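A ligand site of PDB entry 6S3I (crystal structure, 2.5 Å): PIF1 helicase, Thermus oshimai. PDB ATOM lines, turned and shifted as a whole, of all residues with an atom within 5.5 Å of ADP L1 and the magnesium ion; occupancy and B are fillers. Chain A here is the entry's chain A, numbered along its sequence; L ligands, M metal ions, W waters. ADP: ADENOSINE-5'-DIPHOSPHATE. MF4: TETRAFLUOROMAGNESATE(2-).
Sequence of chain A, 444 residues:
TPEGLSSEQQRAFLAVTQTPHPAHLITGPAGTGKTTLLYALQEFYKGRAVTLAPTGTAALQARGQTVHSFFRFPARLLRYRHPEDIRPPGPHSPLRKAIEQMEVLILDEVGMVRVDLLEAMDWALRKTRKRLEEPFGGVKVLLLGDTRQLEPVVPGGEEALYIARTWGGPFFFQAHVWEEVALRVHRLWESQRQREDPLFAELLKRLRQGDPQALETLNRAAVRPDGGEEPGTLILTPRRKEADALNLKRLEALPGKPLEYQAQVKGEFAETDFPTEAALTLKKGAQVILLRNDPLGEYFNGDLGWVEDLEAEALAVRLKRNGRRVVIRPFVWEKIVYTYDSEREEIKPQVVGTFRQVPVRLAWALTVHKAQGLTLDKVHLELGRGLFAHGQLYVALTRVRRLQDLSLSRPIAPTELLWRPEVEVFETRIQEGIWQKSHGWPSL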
ATOM      1  N   LEU A   5      13.907 -21.744   0.586  1.00  0.00           N
ATOM      2  CA  LEU A   5      14.091 -22.822  -0.363  1.00  0.00           C
ATOM      3  C   LEU A   5      15.339 -23.622  -0.014  1.00  0.00           C
ATOM      4  O   LEU A   5      15.347 -24.845  -0.140  1.00  0.00           O
ATOM      5  CB  LEU A   5      14.188 -22.288  -1.794  1.00  0.00           C
ATOM      6  CG  LEU A   5      12.905 -21.735  -2.401  1.00  0.00           C
ATOM      7  CD1 LEU A   5      12.950 -20.208  -2.352  1.00  0.00           C
ATOM      8  CD2 LEU A   5      12.687 -22.231  -3.821  1.00  0.00           C
ATOM      9  N   SER A   6      16.377 -22.941   0.449  1.00  0.00           N
ATOM     10  CA  SER A   6      17.623 -23.621   0.755  1.00  0.00           C
ATOM     11  C   SER A   6      17.430 -24.562   1.937  1.00  0.00           C
ATOM     12  O   SER A   6      16.459 -24.472   2.697  1.00  0.00           O
ATOM     13  CB  SER A   6      18.718 -22.600   1.045  1.00  0.00           C
ATOM     14  OG  SER A   6      19.726 -23.163   1.874  1.00  0.00           O
ATOM     15  N   GLN A   9      18.247 -22.721   5.131  1.00  0.00           N
ATOM     16  CA  GLN A   9      17.116 -21.815   5.282  1.00  0.00           C
ATOM     17  C   GLN A   9      15.895 -22.559   5.818  1.00  0.00           C
ATOM     18  O   GLN A   9      15.236 -22.092   6.746  1.00  0.00           O
ATOM     19  CB  GLN A   9      16.794 -21.163   3.944  1.00  0.00           C
ATOM     20  CG  GLN A   9      17.458 -19.834   3.715  1.00  0.00           C
ATOM     21  CD  GLN A   9      17.312 -19.397   2.281  1.00  0.00           C
ATOM     22  OE1 GLN A   9      16.865 -20.173   1.432  1.00  0.00           O
ATOM     23  NE2 GLN A   9      17.656 -18.159   2.001  1.00  0.00           N
ATOM     24  N   PRO A  29      27.073 -15.315   7.171  1.00  0.00           N
ATOM     25  CA  PRO A  29      27.775 -14.333   6.329  1.00  0.00           C
ATOM     26  C   PRO A  29      26.858 -13.630   5.350  1.00  0.00           C
ATOM     27  O   PRO A  29      25.666 -13.951   5.254  1.00  0.00           O
ATOM     28  CB  PRO A  29      28.816 -15.187   5.585  1.00  0.00           C
ATOM     29  CG  PRO A  29      28.937 -16.438   6.375  1.00  0.00           C
ATOM     30  CD  PRO A  29      27.597 -16.673   6.990  1.00  0.00           C
ATOM     31  N   ALA A  30      27.387 -12.658   4.609  1.00  0.00           N
ATOM     32  CA  ALA A  30      26.554 -11.833   3.752  1.00  0.00           C
ATOM     33  C   ALA A  30      26.112 -12.615   2.525  1.00  0.00           C
ATOM     34  O   ALA A  30      26.907 -13.322   1.899  1.00  0.00           O
ATOM     35  CB  ALA A  30      27.309 -10.581   3.327  1.00  0.00           C
ATOM     36  N   GLY A  31      24.835 -12.477   2.188  1.00  0.00           N
ATOM     37  CA  GLY A  31      24.250 -13.126   1.038  1.00  0.00           C
ATOM     38  C   GLY A  31      23.827 -14.559   1.257  1.00  0.00           C
ATOM     39  O   GLY A  31      23.463 -15.241   0.289  1.00  0.00           O
ATOM     40  N   THR A  32      23.844 -15.043   2.506  1.00  0.00           N
ATOM     41  CA  THR A  32      23.451 -16.412   2.810  1.00  0.00           C
ATOM     42  C   THR A  32      21.940 -16.623   2.798  1.00  0.00           C
ATOM     43  O   THR A  32      21.485 -17.770   2.856  1.00  0.00           O
ATOM     44  CB  THR A  32      24.009 -16.848   4.169  1.00  0.00           C
ATOM     45  OG1 THR A  32      23.686 -15.876   5.166  1.00  0.00           O
ATOM     46  CG2 THR A  32      25.525 -17.009   4.090  1.00  0.00           C
ATOM     47  N   GLY A  33      21.154 -15.550   2.719  1.00  0.00           N
ATOM     48  CA  GLY A  33      19.720 -15.677   2.648  1.00  0.00           C
ATOM     49  C   GLY A  33      18.942 -15.347   3.907  1.00  0.00           C
ATOM     50  O   GLY A  33      17.818 -15.840   4.057  1.00  0.00           O
ATOM     51  N   LYS A  34      19.509 -14.541   4.806  1.00  0.00           N
ATOM     52  CA  LYS A  34      18.785 -14.210   6.031  1.00  0.00           C
ATOM     53  C   LYS A  34      17.499 -13.452   5.712  1.00  0.00           C
ATOM     54  O   LYS A  34      16.401 -13.860   6.123  1.00  0.00           O
ATOM     55  CB  LYS A  34      19.667 -13.370   6.961  1.00  0.00           C
ATOM     56  CG  LYS A  34      20.547 -14.162   7.890  1.00  0.00           C
ATOM     57  CD  LYS A  34      22.017 -13.944   7.593  1.00  0.00           C
ATOM     58  CE  LYS A  34      22.463 -12.503   7.786  1.00  0.00           C
ATOM     59  NZ  LYS A  34      23.443 -12.181   6.706  1.00  0.00           N
ATOM     60  N   THR A  35      17.620 -12.338   4.979  1.00  0.00           N
ATOM     61  CA  THR A  35      16.452 -11.513   4.674  1.00  0.00           C
ATOM     62  C   THR A  35      15.457 -12.247   3.789  1.00  0.00           C
ATOM     63  O   THR A  35      14.251 -11.962   3.852  1.00  0.00           O
ATOM     64  CB  THR A  35      16.921 -10.211   4.010  1.00  0.00           C
ATOM     65  OG1 THR A  35      17.879  -9.558   4.857  1.00  0.00           O
ATOM     66  CG2 THR A  35      15.750  -9.267   3.786  1.00  0.00           C
ATOM     67  N   THR A  36      15.921 -13.180   2.957  1.00  0.00           N
ATOM     68  CA  THR A  36      14.999 -13.990   2.171  1.00  0.00           C
ATOM     69  C   THR A  36      14.215 -14.952   3.057  1.00  0.00           C
ATOM     70  O   THR A  36      13.017 -15.168   2.835  1.00  0.00           O
ATOM     71  CB  THR A  36      15.758 -14.758   1.093  1.00  0.00           C
ATOM     72  OG1 THR A  36      16.462 -13.829   0.263  1.00  0.00           O
ATOM     73  CG2 THR A  36      14.812 -15.564   0.243  1.00  0.00           C
ATOM     74  N   LEU A  37      14.870 -15.530   4.067  1.00  0.00           N
ATOM     75  CA  LEU A  37      14.146 -16.349   5.035  1.00  0.00           C
ATOM     76  C   LEU A  37      13.141 -15.512   5.801  1.00  0.00           C
ATOM     77  O   LEU A  37      12.059 -16.003   6.149  1.00  0.00           O
ATOM     78  CB  LEU A  37      15.141 -16.996   6.002  1.00  0.00           C
ATOM     79  CG  LEU A  37      14.561 -17.811   7.159  1.00  0.00           C
ATOM     80  CD1 LEU A  37      13.545 -18.827   6.675  1.00  0.00           C
ATOM     81  CD2 LEU A  37      15.680 -18.507   7.928  1.00  0.00           C
ATOM     82  N   GLN A  61      14.159  -3.074   2.478  1.00  0.00           N
ATOM     83  CA  GLN A  61      14.587  -4.347   1.923  1.00  0.00           C
ATOM     84  C   GLN A  61      13.888  -5.516   2.602  1.00  0.00           C
ATOM     85  O   GLN A  61      13.615  -6.540   1.966  1.00  0.00           O
ATOM     86  CB  GLN A  61      16.117  -4.465   2.057  1.00  0.00           C
ATOM     87  CG  GLN A  61      16.719  -5.822   1.702  1.00  0.00           C
ATOM     88  CD  GLN A  61      16.746  -6.096   0.213  1.00  0.00           C
ATOM     89  OE1 GLN A  61      16.638  -5.179  -0.599  1.00  0.00           O
ATOM     90  NE2 GLN A  61      16.882  -7.373  -0.152  1.00  0.00           N
ATOM     91  N   ASP A 108      15.561  -7.428  11.514  1.00  0.00           N
ATOM     92  CA  ASP A 108      16.628  -7.727  10.557  1.00  0.00           C
ATOM     93  C   ASP A 108      17.796  -6.767  10.744  1.00  0.00           C
ATOM     94  O   ASP A 108      17.674  -5.695  11.342  1.00  0.00           O
ATOM     95  CB  ASP A 108      16.096  -7.638   9.125  1.00  0.00           C
ATOM     96  CG  ASP A 108      16.983  -8.380   8.116  1.00  0.00           C
ATOM     97  OD1 ASP A 108      18.009  -8.962   8.516  1.00  0.00           O
ATOM     98  OD2 ASP A 108      16.641  -8.390   6.904  1.00  0.00           O
ATOM     99  N   GLU A 109      18.951  -7.171  10.218  1.00  0.00           N
ATOM    100  CA  GLU A 109      20.206  -6.439  10.377  1.00  0.00           C
ATOM    101  C   GLU A 109      20.436  -6.129  11.861  1.00  0.00           C
ATOM    102  O   GLU A 109      20.646  -4.984  12.253  1.00  0.00           O
ATOM    103  CB  GLU A 109      20.215  -5.135   9.560  1.00  0.00           C
ATOM    104  CG  GLU A 109      20.354  -5.262   8.036  1.00  0.00           C
ATOM    105  CD  GLU A 109      21.531  -6.100   7.586  1.00  0.00           C
ATOM    106  OE1 GLU A 109      22.408  -6.404   8.411  1.00  0.00           O
ATOM    107  OE2 GLU A 109      21.583  -6.447   6.383  1.00  0.00           O
ATOM    108  N   GLN A 192      24.048 -17.559  -1.100  1.00  0.00           N
ATOM    109  CA  GLN A 192      23.077 -17.568  -2.181  1.00  0.00           C
ATOM    110  C   GLN A 192      23.205 -16.370  -3.103  1.00  0.00           C
ATOM    111  O   GLN A 192      22.928 -16.502  -4.298  1.00  0.00           O
ATOM    112  CB  GLN A 192      21.654 -17.595  -1.602  1.00  0.00           C
ATOM    113  CG  GLN A 192      21.302 -18.920  -0.929  1.00  0.00           C
ATOM    114  CD  GLN A 192      20.946 -19.995  -1.929  1.00  0.00           C
ATOM    115  OE1 GLN A 192      20.519 -19.706  -3.052  1.00  0.00           O
ATOM    116  NE2 GLN A 192      21.103 -21.253  -1.534  1.00  0.00           N
ATOM    117  N   ARG A 193      23.617 -15.215  -2.594  1.00  0.00           N
ATOM    118  CA  ARG A 193      23.826 -14.057  -3.453  1.00  0.00           C
ATOM    119  C   ARG A 193      24.921 -14.338  -4.475  1.00  0.00           C
ATOM    120  O   ARG A 193      24.803 -13.959  -5.650  1.00  0.00           O
ATOM    121  CB  ARG A 193      24.178 -12.818  -2.631  1.00  0.00           C
ATOM    122  CG  ARG A 193      24.661 -11.647  -3.488  1.00  0.00           C
ATOM    123  CD  ARG A 193      24.787 -10.362  -2.684  1.00  0.00           C
ATOM    124  NE  ARG A 193      23.514  -9.911  -2.124  1.00  0.00           N
ATOM    125  CZ  ARG A 193      23.315  -9.550  -0.854  1.00  0.00           C
ATOM    126  NH1 ARG A 193      24.313  -9.559   0.022  1.00  0.00           N
ATOM    127  NH2 ARG A 193      22.111  -9.157  -0.469  1.00  0.00           N
ATOM    128  N   ARG A 195      26.024 -17.389  -5.415  1.00  0.00           N
ATOM    129  CA  ARG A 195      25.984 -18.797  -5.801  1.00  0.00           C
ATOM    130  C   ARG A 195      26.477 -19.018  -7.228  1.00  0.00           C
ATOM    131  O   ARG A 195      26.802 -20.151  -7.589  1.00  0.00           O
ATOM    132  CB  ARG A 195      24.553 -19.328  -5.662  1.00  0.00           C
ATOM    133  CG  ARG A 195      23.620 -18.874  -6.785  1.00  0.00           C
ATOM    134  CD  ARG A 195      22.141 -19.040  -6.430  1.00  0.00           C
ATOM    135  NE  ARG A 195      21.486 -20.032  -7.266  1.00  0.00           N
ATOM    136  CZ  ARG A 195      21.023 -19.800  -8.505  1.00  0.00           C
ATOM    137  NH1 ARG A 195      21.156 -18.597  -9.049  1.00  0.00           N
ATOM    138  NH2 ARG A 195      20.446 -20.775  -9.187  1.00  0.00           N
ATOM    139  N   GLY A 373      22.698  -4.749   3.350  1.00  0.00           N
ATOM    140  CA  GLY A 373      21.455  -5.471   3.184  1.00  0.00           C
ATOM    141  C   GLY A 373      21.000  -5.593   1.746  1.00  0.00           C
ATOM    142  O   GLY A 373      20.148  -6.444   1.450  1.00  0.00           O
ATOM    143  N   THR A 375      21.125  -6.156  -2.429  1.00  0.00           N
ATOM    144  CA  THR A 375      21.761  -6.876  -3.533  1.00  0.00           C
ATOM    145  C   THR A 375      21.804  -5.928  -4.731  1.00  0.00           C
ATOM    146  O   THR A 375      20.760  -5.474  -5.204  1.00  0.00           O
ATOM    147  CB  THR A 375      20.992  -8.159  -3.859  1.00  0.00           C
ATOM    148  OG1 THR A 375      21.024  -9.024  -2.711  1.00  0.00           O
ATOM    149  CG2 THR A 375      21.626  -8.874  -5.045  1.00  0.00           C
ATOM    150  N   ARG A 399      28.026  -6.759  -1.834  1.00  0.00           N
ATOM    151  CA  ARG A 399      26.757  -6.316  -2.406  1.00  0.00           C
ATOM    152  C   ARG A 399      26.506  -6.897  -3.793  1.00  0.00           C
ATOM    153  O   ARG A 399      25.367  -6.829  -4.278  1.00  0.00           O
ATOM    154  CB  ARG A 399      26.732  -4.783  -2.466  1.00  0.00           C
ATOM    155  CG  ARG A 399      26.968  -4.113  -1.118  1.00  0.00           C
ATOM    156  CD  ARG A 399      25.887  -4.502  -0.121  1.00  0.00           C
ATOM    157  NE  ARG A 399      26.279  -5.630   0.739  1.00  0.00           N
ATOM    158  CZ  ARG A 399      25.418  -6.476   1.300  1.00  0.00           C
ATOM    159  NH1 ARG A 399      24.116  -6.358   1.089  1.00  0.00           N
ATOM    160  NH2 ARG A 399      25.875  -7.462   2.069  1.00  0.00           N
ATOM    161  N   ARG A 401      26.950 -10.073  -6.908  1.00  0.00           N
ATOM    162  CA  ARG A 401      26.873 -11.512  -7.037  1.00  0.00           C
ATOM    163  C   ARG A 401      28.088 -12.121  -7.711  1.00  0.00           C
ATOM    164  O   ARG A 401      28.479 -13.240  -7.369  1.00  0.00           O
ATOM    165  CB  ARG A 401      25.629 -11.906  -7.854  1.00  0.00           C
ATOM    166  CG  ARG A 401      24.362 -11.175  -7.441  1.00  0.00           C
ATOM    167  CD  ARG A 401      24.103  -9.973  -8.336  1.00  0.00           C
ATOM    168  NE  ARG A 401      22.754  -9.455  -8.181  1.00  0.00           N
ATOM    169  CZ  ARG A 401      21.654 -10.099  -8.584  1.00  0.00           C
ATOM    170  NH1 ARG A 401      21.749 -11.285  -9.153  1.00  0.00           N
ATOM    171  NH2 ARG A 401      20.458  -9.549  -8.406  1.00  0.00           N
HETATM  172  PB  ADP L   1      21.198 -11.844   3.263  1.00  0.00           P
HETATM  173  O1B ADP L   1      22.260 -10.952   2.672  1.00  0.00           O
HETATM  174  O2B ADP L   1      21.756 -12.829   4.258  1.00  0.00           O
HETATM  175  O3B ADP L   1      19.969 -11.087   3.736  1.00  0.00           O
HETATM  176  PA  ADP L   1      19.555 -12.142   1.010  1.00  0.00           P
HETATM  177  O1A ADP L   1      19.937 -10.697   0.808  1.00  0.00           O
HETATM  178  O2A ADP L   1      18.170 -12.523   1.494  1.00  0.00           O
HETATM  179  O3A ADP L   1      20.640 -12.748   2.044  1.00  0.00           O
HETATM  180  O5' ADP L   1      19.798 -12.971  -0.351  1.00  0.00           O
HETATM  181  C5' ADP L   1      20.672 -12.456  -1.361  1.00  0.00           C
HETATM  182  C4' ADP L   1      20.200 -12.860  -2.754  1.00  0.00           C
HETATM  183  O4' ADP L   1      20.249 -14.282  -2.816  1.00  0.00           O
HETATM  184  C3' ADP L   1      18.791 -12.417  -3.128  1.00  0.00           C
HETATM  185  O3' ADP L   1      18.805 -11.603  -4.299  1.00  0.00           O
HETATM  186  C2' ADP L   1      17.986 -13.689  -3.374  1.00  0.00           C
HETATM  187  O2' ADP L   1      17.291 -13.700  -4.607  1.00  0.00           O
HETATM  188  C1' ADP L   1      19.050 -14.794  -3.392  1.00  0.00           C
HETATM  189  N9  ADP L   1      18.607 -15.987  -2.667  1.00  0.00           N
HETATM  190  C8  ADP L   1      18.521 -16.160  -1.328  1.00  0.00           C
HETATM  191  N7  ADP L   1      18.073 -17.416  -1.053  1.00  0.00           N
HETATM  192  C5  ADP L   1      17.877 -18.049  -2.228  1.00  0.00           C
HETATM  193  C6  ADP L   1      17.408 -19.382  -2.680  1.00  0.00           C
HETATM  194  N6  ADP L   1      17.059 -20.328  -1.782  1.00  0.00           N
HETATM  195  N1  ADP L   1      17.354 -19.615  -4.009  1.00  0.00           N
HETATM  196  C2  ADP L   1      17.702 -18.694  -4.931  1.00  0.00           C
HETATM  197  N3  ADP L   1      18.127 -17.472  -4.583  1.00  0.00           N
HETATM  198  C4  ADP L   1      18.230 -17.097  -3.277  1.00  0.00           C
HETATM  199 MG   MF4 L   2      23.075  -8.805   4.224  1.00  0.00          MG
HETATM  200  F1  MF4 L   2      21.279  -8.750   4.253  1.00  0.00           F
HETATM  201  F2  MF4 L   2      23.716  -7.263   4.832  1.00  0.00           F
HETATM  202  F3  MF4 L   2      23.768 -10.017   5.330  1.00  0.00           F
HETATM  203  F4  MF4 L   2      23.833  -8.990   2.608  1.00  0.00           F
HETATM  204 MG    MG M   1      19.392  -8.676   4.407  1.00  0.00          MG
HETATM  205  O   HOH W   1      18.924  -8.627   2.466  1.00  0.00           O
HETATM  206  O   HOH W   2      19.629  -6.896   5.416  1.00  0.00           O
HETATM  207  O   HOH W   3      19.343  -9.578   6.580  1.00  0.00           O
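The backbone NH (N) of Thr 35 sits close to an oxygen (O3B) of ADP L1 (2.9 Å).
N of Thr 36 is in hydrogen-bond range of O2A of ADP L1 (2.8 Å).
An oxygen (O2A) of ADP L1 lies within hydrogen-bond range of the side-chain hydroxyl (OG1) of Thr 36 (2.5 Å).
An oxygen (O2B) of ADP L1 sits at hydrogen-bond distance from the backbone NH (N) of Lys 34 (2.9 Å).
The side-chain amino group (NZ) of Lys 34 lies within salt-bridge range of an oxygen (O2B) of ADP L1.
The backbone NH (N) of Gly 33 lies within hydrogen-bond range of an oxygen (O3A) of ADP L1 (2.9 Å).
The guanidinium group of Arg 193 is in salt-bridge range of an oxygen (O1A) of ADP L1 (3.0 Å).
The backbone NH (N) of Gly 31 sits at hydrogen-bond distance from an oxygen (O1B) of ADP L1 (3.0 Å).
OE1 of Gln 192 sits close to N1 of ADP L1, 3.3 Å away.
The side-chain amide nitrogen of Gln 9 lies within hydrogen-bond range of a nitrogen (N7) of ADP L1, 3.2 Å away.
The side-chain amino group of Lys 34 sits at hydrogen-bond distance from a fluorine (F3) of MF4 L2, 2.6 Å away.
NH1 of Arg 193 is in hydrogen-bond range of F4 of MF4 L2.
The backbone NH (N) of Gly 373 lies within hydrogen-bond range of a fluorine (F2) of MF4 L2 (3.1 Å).
The guanidinium group (NH2) of Arg 399 is in hydrogen-bond range of a fluorine (F4) of MF4 L2 (2.6 Å).
CB of Leu 5 touches N6 of ADP L1, at 3.5 Å.
N of Ser 6 touches N6 of ADP L1, 3.5 Å away.
N of Thr 32 touches O2B of ADP L1 (3.5 Å).
OG1 of Thr 375 touches C5' of ADP L1 (3.7 Å).
The nearest printed residue that does not touch ADP L1 is Pro 29 (4.2 Å).
Merely in contact with the magnesium ion: Glu 109, Asp 108 and Gly 373.
Within 4 Å of the magnesium ion: Thr 35, Asp 108, Glu 109 and Gly 373.
The side-chain carboxylate of Asp 108 sits close to the side-chain hydroxyl of Thr 35.
NZ of Lys 34 sits at hydrogen-bond distance from O of Pro 29 (3.2 Å).
O of Gly 33 lies within hydrogen-bond range of NE2 of Gln 9, at 3.1 Å.
O of Gly 31 lies within hydrogen-bond range of N of Arg 193 (2.9 Å).
NH2 of Arg 193 lies within hydrogen-bond range of OG1 of Thr 375, 2.5 Å away.
The backbone NH of Gln 192 lies within hydrogen-bond range of the backbone carbonyl oxygen of Gly 31 (2.8 Å).
The side-chain amide oxygen (OE1) of Gln 9 lies within hydrogen-bond range of the backbone NH (N) of Ser 6, 3.0 Å away.
The backbone carbonyl oxygen (O) of Pro 29 is in hydrogen-bond range of the side-chain hydroxyl (OG1) of Thr 32 (2.8 Å).
Water W1 bridges O of Gly 373 (2.7 Å) and O1A of ADP L1 (2.8 Å).
The magnesium ion is bound by OG1 of Thr 35 (1.8 Å), F1 of MF4 L2 (1.9 Å), water W1 (2.0 Å), water W2 (2.1 Å), water W3 (2.4 Å) and O3B of ADP L1 (2.6 Å).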
